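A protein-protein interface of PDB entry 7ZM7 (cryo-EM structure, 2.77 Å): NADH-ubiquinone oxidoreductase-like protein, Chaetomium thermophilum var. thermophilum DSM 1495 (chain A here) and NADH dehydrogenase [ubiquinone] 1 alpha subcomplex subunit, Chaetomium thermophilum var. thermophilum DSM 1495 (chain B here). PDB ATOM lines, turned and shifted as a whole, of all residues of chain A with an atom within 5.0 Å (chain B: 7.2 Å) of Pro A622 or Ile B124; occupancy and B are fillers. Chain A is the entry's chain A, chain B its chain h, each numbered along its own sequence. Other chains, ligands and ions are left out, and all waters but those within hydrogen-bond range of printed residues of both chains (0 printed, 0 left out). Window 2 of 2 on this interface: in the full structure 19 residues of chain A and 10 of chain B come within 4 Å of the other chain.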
ATOM      1  N   LEU A 279     -18.596  25.591   6.782  1.00  0.00           N
ATOM      2  CA  LEU A 279     -18.449  24.387   7.630  1.00  0.00           C
ATOM      3  C   LEU A 279     -19.522  24.359   8.709  1.00  0.00           C
ATOM      4  O   LEU A 279     -19.433  23.495   9.596  1.00  0.00           O
ATOM      5  CB  LEU A 279     -17.039  24.374   8.233  1.00  0.00           C
ATOM      6  CG  LEU A 279     -16.605  25.629   8.990  1.00  0.00           C
ATOM      7  CD1 LEU A 279     -16.859  25.481  10.481  1.00  0.00           C
ATOM      8  CD2 LEU A 279     -15.134  25.914   8.743  1.00  0.00           C
ATOM      9  N   LEU A 308     -25.434  20.261  16.520  1.00  0.00           N
ATOM     10  CA  LEU A 308     -24.313  19.655  15.766  1.00  0.00           C
ATOM     11  C   LEU A 308     -23.044  20.500  15.896  1.00  0.00           C
ATOM     12  O   LEU A 308     -22.040  20.144  15.270  1.00  0.00           O
ATOM     13  CB  LEU A 308     -24.751  19.545  14.308  1.00  0.00           C
ATOM     14  CG  LEU A 308     -25.619  18.336  13.980  1.00  0.00           C
ATOM     15  CD1 LEU A 308     -26.104  18.402  12.544  1.00  0.00           C
ATOM     16  CD2 LEU A 308     -24.846  17.051  14.222  1.00  0.00           C
ATOM     17  N   LYS A 309     -23.089  21.586  16.659  1.00  0.00           N
ATOM     18  CA  LYS A 309     -21.902  22.452  16.862  1.00  0.00           C
ATOM     19  C   LYS A 309     -21.718  22.801  18.344  1.00  0.00           C
ATOM     20  O   LYS A 309     -21.214  23.900  18.618  1.00  0.00           O
ATOM     21  CB  LYS A 309     -22.070  23.736  16.055  1.00  0.00           C
ATOM     22  CG  LYS A 309     -23.346  24.521  16.327  1.00  0.00           C
ATOM     23  CD  LYS A 309     -23.368  25.858  15.621  1.00  0.00           C
ATOM     24  CE  LYS A 309     -24.461  26.772  16.129  1.00  0.00           C
ATOM     25  NZ  LYS A 309     -24.297  27.066  17.571  1.00  0.00           N
ATOM     26  N   ARG A 312     -19.190  18.614  20.540  1.00  0.00           N
ATOM     27  CA  ARG A 312     -18.625  17.660  19.609  1.00  0.00           C
ATOM     28  C   ARG A 312     -17.305  17.103  20.112  1.00  0.00           C
ATOM     29  O   ARG A 312     -16.501  17.815  20.715  1.00  0.00           O
ATOM     30  CB  ARG A 312     -18.428  18.320  18.252  1.00  0.00           C
ATOM     31  CG  ARG A 312     -19.646  19.026  17.750  1.00  0.00           C
ATOM     32  CD  ARG A 312     -20.640  18.056  17.175  1.00  0.00           C
ATOM     33  NE  ARG A 312     -20.000  16.920  16.536  1.00  0.00           N
ATOM     34  CZ  ARG A 312     -19.857  16.780  15.231  1.00  0.00           C
ATOM     35  NH1 ARG A 312     -20.292  17.718  14.411  1.00  0.00           N
ATOM     36  NH2 ARG A 312     -19.269  15.704  14.748  1.00  0.00           N
ATOM     37  N   LEU A 313     -17.092  15.816  19.862  1.00  0.00           N
ATOM     38  CA  LEU A 313     -15.799  15.189  20.087  1.00  0.00           C
ATOM     39  C   LEU A 313     -14.906  15.490  18.901  1.00  0.00           C
ATOM     40  O   LEU A 313     -15.229  15.120  17.771  1.00  0.00           O
ATOM     41  CB  LEU A 313     -15.951  13.686  20.257  1.00  0.00           C
ATOM     42  CG  LEU A 313     -17.127  13.226  21.091  1.00  0.00           C
ATOM     43  CD1 LEU A 313     -17.285  11.750  20.978  1.00  0.00           C
ATOM     44  CD2 LEU A 313     -16.912  13.635  22.505  1.00  0.00           C
ATOM     45  N   THR A 314     -13.792  16.163  19.145  1.00  0.00           N
ATOM     46  CA  THR A 314     -12.926  16.564  18.058  1.00  0.00           C
ATOM     47  C   THR A 314     -11.520  16.005  18.137  1.00  0.00           C
ATOM     48  O   THR A 314     -10.736  16.253  17.219  1.00  0.00           O
ATOM     49  CB  THR A 314     -12.859  18.098  17.965  1.00  0.00           C
ATOM     50  OG1 THR A 314     -12.319  18.637  19.175  1.00  0.00           O
ATOM     51  CG2 THR A 314     -14.230  18.678  17.725  1.00  0.00           C
ATOM     52  N   GLU A 600     -21.698  14.932   7.870  1.00  0.00           N
ATOM     53  CA  GLU A 600     -20.427  14.930   7.160  1.00  0.00           C
ATOM     54  C   GLU A 600     -19.949  13.524   6.815  1.00  0.00           C
ATOM     55  O   GLU A 600     -18.752  13.305   6.662  1.00  0.00           O
ATOM     56  CB  GLU A 600     -19.343  15.687   7.932  1.00  0.00           C
ATOM     57  CG  GLU A 600     -18.929  15.145   9.266  1.00  0.00           C
ATOM     58  CD  GLU A 600     -19.729  15.746  10.384  1.00  0.00           C
ATOM     59  OE1 GLU A 600     -20.791  16.306  10.088  1.00  0.00           O
ATOM     60  OE2 GLU A 600     -19.289  15.691  11.557  1.00  0.00           O
ATOM     61  N   GLY A 620     -17.395  18.944   5.971  1.00  0.00           N
ATOM     62  CA  GLY A 620     -16.328  18.017   6.265  1.00  0.00           C
ATOM     63  C   GLY A 620     -16.252  17.692   7.739  1.00  0.00           C
ATOM     64  O   GLY A 620     -17.020  18.194   8.552  1.00  0.00           O
ATOM     65  N   LEU A 621     -15.289  16.842   8.078  1.00  0.00           N
ATOM     66  CA  LEU A 621     -15.092  16.408   9.452  1.00  0.00           C
ATOM     67  C   LEU A 621     -14.522  17.543  10.298  1.00  0.00           C
ATOM     68  O   LEU A 621     -13.625  18.257   9.853  1.00  0.00           O
ATOM     69  CB  LEU A 621     -14.132  15.220   9.498  1.00  0.00           C
ATOM     70  CG  LEU A 621     -14.421  13.923   8.742  1.00  0.00           C
ATOM     71  CD1 LEU A 621     -13.177  13.120   8.600  1.00  0.00           C
ATOM     72  CD2 LEU A 621     -15.431  13.145   9.470  1.00  0.00           C
ATOM     73  N   PRO A 622     -15.009  17.728  11.524  1.00  0.00           N
ATOM     74  CA  PRO A 622     -14.451  18.766  12.396  1.00  0.00           C
ATOM     75  C   PRO A 622     -13.282  18.248  13.224  1.00  0.00           C
ATOM     76  O   PRO A 622     -13.324  17.138  13.755  1.00  0.00           O
ATOM     77  CB  PRO A 622     -15.637  19.145  13.288  1.00  0.00           C
ATOM     78  CG  PRO A 622     -16.398  17.912  13.391  1.00  0.00           C
ATOM     79  CD  PRO A 622     -16.264  17.195  12.066  1.00  0.00           C
ATOM     80  N   GLY A 623     -12.245  19.070  13.339  1.00  0.00           N
ATOM     81  CA  GLY A 623     -11.101  18.724  14.165  1.00  0.00           C
ATOM     82  C   GLY A 623     -10.363  17.525  13.631  1.00  0.00           C
ATOM     83  O   GLY A 623     -10.035  17.448  12.449  1.00  0.00           O
ATOM     84  N   ALA A 624     -10.077  16.580  14.519  1.00  0.00           N
ATOM     85  CA  ALA A 624      -9.380  15.353  14.174  1.00  0.00           C
ATOM     86  C   ALA A 624     -10.309  14.164  14.078  1.00  0.00           C
ATOM     87  O   ALA A 624      -9.837  13.028  14.093  1.00  0.00           O
ATOM     88  CB  ALA A 624      -8.283  15.058  15.192  1.00  0.00           C
ATOM     89  N   ALA A 625     -11.612  14.391  13.995  1.00  0.00           N
ATOM     90  CA  ALA A 625     -12.544  13.289  13.851  1.00  0.00           C
ATOM     91  C   ALA A 625     -12.231  12.500  12.588  1.00  0.00           C
ATOM     92  O   ALA A 625     -11.521  12.961  11.697  1.00  0.00           O
ATOM     93  CB  ALA A 625     -13.977  13.812  13.818  1.00  0.00           C
ATOM     94  N   GLN B 121     -17.163  34.461  17.039  1.00  0.00           N
ATOM     95  CA  GLN B 121     -16.719  33.352  17.873  1.00  0.00           C
ATOM     96  C   GLN B 121     -16.423  32.106  17.035  1.00  0.00           C
ATOM     97  O   GLN B 121     -16.905  31.971  15.913  1.00  0.00           O
ATOM     98  CB  GLN B 121     -17.780  33.027  18.915  1.00  0.00           C
ATOM     99  CG  GLN B 121     -18.054  34.129  19.891  1.00  0.00           C
ATOM    100  CD  GLN B 121     -17.218  34.036  21.145  1.00  0.00           C
ATOM    101  OE1 GLN B 121     -15.996  34.051  21.096  1.00  0.00           O
ATOM    102  NE2 GLN B 121     -17.875  33.953  22.278  1.00  0.00           N
ATOM    103  N   PRO B 122     -15.611  31.188  17.555  1.00  0.00           N
ATOM    104  CA  PRO B 122     -15.349  29.938  16.829  1.00  0.00           C
ATOM    105  C   PRO B 122     -16.621  29.149  16.587  1.00  0.00           C
ATOM    106  O   PRO B 122     -17.500  29.073  17.447  1.00  0.00           O
ATOM    107  CB  PRO B 122     -14.395  29.178  17.745  1.00  0.00           C
ATOM    108  CG  PRO B 122     -13.944  30.139  18.753  1.00  0.00           C
ATOM    109  CD  PRO B 122     -14.816  31.310  18.783  1.00  0.00           C
ATOM    110  N   LYS B 123     -16.692  28.534  15.405  1.00  0.00           N
ATOM    111  CA  LYS B 123     -17.949  27.966  14.937  1.00  0.00           C
ATOM    112  C   LYS B 123     -18.397  26.790  15.786  1.00  0.00           C
ATOM    113  O   LYS B 123     -19.534  26.763  16.269  1.00  0.00           O
ATOM    114  CB  LYS B 123     -17.810  27.546  13.484  1.00  0.00           C
ATOM    115  CG  LYS B 123     -17.520  28.701  12.581  1.00  0.00           C
ATOM    116  CD  LYS B 123     -18.707  29.627  12.519  1.00  0.00           C
ATOM    117  CE  LYS B 123     -18.455  30.757  11.544  1.00  0.00           C
ATOM    118  NZ  LYS B 123     -19.600  31.698  11.500  1.00  0.00           N
ATOM    119  N   ILE B 124     -17.529  25.816  15.999  1.00  0.00           N
ATOM    120  CA  ILE B 124     -17.926  24.563  16.614  1.00  0.00           C
ATOM    121  C   ILE B 124     -17.355  24.517  18.015  1.00  0.00           C
ATOM    122  O   ILE B 124     -16.151  24.698  18.210  1.00  0.00           O
ATOM    123  CB  ILE B 124     -17.473  23.355  15.780  1.00  0.00           C
ATOM    124  CG1 ILE B 124     -18.163  23.392  14.419  1.00  0.00           C
ATOM    125  CG2 ILE B 124     -17.841  22.076  16.476  1.00  0.00           C
ATOM    126  CD1 ILE B 124     -17.627  22.425  13.422  1.00  0.00           C
ATOM    127  N   GLN B 125     -18.228  24.304  18.985  1.00  0.00           N
ATOM    128  CA  GLN B 125     -17.847  24.117  20.367  1.00  0.00           C
ATOM    129  C   GLN B 125     -17.513  22.652  20.597  1.00  0.00           C
ATOM    130  O   GLN B 125     -18.253  21.766  20.171  1.00  0.00           O
ATOM    131  CB  GLN B 125     -18.971  24.570  21.291  1.00  0.00           C
ATOM    132  CG  GLN B 125     -19.223  26.054  21.241  1.00  0.00           C
ATOM    133  CD  GLN B 125     -20.358  26.475  22.146  1.00  0.00           C
ATOM    134  OE1 GLN B 125     -21.009  25.640  22.770  1.00  0.00           O
ATOM    135  NE2 GLN B 125     -20.607  27.778  22.217  1.00  0.00           N
ATOM    136  N   SER B 126     -16.395  22.410  21.255  1.00  0.00           N
ATOM    137  CA  SER B 126     -15.943  21.064  21.548  1.00  0.00           C
ATOM    138  C   SER B 126     -16.352  20.656  22.955  1.00  0.00           C
ATOM    139  O   SER B 126     -16.488  21.484  23.854  1.00  0.00           O
ATOM    140  CB  SER B 126     -14.431  20.960  21.383  1.00  0.00           C
ATOM    141  OG  SER B 126     -13.995  19.652  21.651  1.00  0.00           O
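Leu A279 touches Lys B123 (CD1 to CB, 3.8 Å).
Lys A309 touches Lys B123 (CB to O, 3.95 Å).
Lys A309 touches Ile B124.
Ile B124 touches Arg A312.
CD1 of Ile B124 touches CB of Pro A622, 3.8 Å away.
Printed residues of chain A that touch a printed residue of chain B: Leu A279, Lys A309, Arg A312, Thr A314 and Pro A622.
Of the 6 printed residues of chain B, 4 touch a printed residue of chain A.
Printed residues of chain B that touch a printed residue of chain A: Lys B123, Ile B124, Gln B125 and Ser B126.
Among the printed residues, 9 pairs touch across the chains.
OE2 of Glu A600 lies within salt-bridge range of NH2 of Arg A312 (3.2 Å).
The backbone carbonyl oxygen (O) of Leu A308 is in hydrogen-bond range of the guanidinium group (NH1) of Arg A312, 3.1 Å away.
The backbone NH of Ala A624 sits at hydrogen-bond distance from the backbone carbonyl oxygen of Thr A314 (2.8 Å).
Pro A622 touches just one residue of chain B: Ile B124.
Ile B124 touches just these residues of chain A: Lys A309, Arg A312 and Pro A622.
Printed residues of chain A within 4 Å of Lys B123: Leu A279 and Lys A309.
Printed residues of chain B within 4 Å of Arg A312: Ile B124, Gln B125 and Ser B126.
Of the printed residues of chain B, Lys A309 touches Lys B123 (3.95 Å), Ile B124 (3.9 Å) and Gln B125 (3.0 Å).
Of the printed residues of chain A, Gln B125 touches Lys A309 (3.0 Å) and Arg A312 (3.3 Å).
Of the printed residues of chain B, Leu A279 touches Lys B123.
Ala A624 touches none of the printed residues of chain B.
The nearest printed residue of chain B that does not touch Pro A622 is Gln B125 (7.8 Å).
The nearest printed residue of chain A that does not touch Ser B126 is Leu A313 (5.1 Å).
The backbone NH (N) of Gln B125 is in hydrogen-bond range of the backbone carbonyl oxygen (O) of Lys A309 (3.0 Å).
The side-chain hydroxyl (OG) of Ser B126 is in hydrogen-bond range of the side-chain hydroxyl (OG1) of Thr A314 (3.2 Å).
OG of Ser B126 sits at hydrogen-bond distance from O of Arg A312 (3.2 Å).
N of Arg A312 lies within hydrogen-bond range of O of Gln B125, 3.3 Å away.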
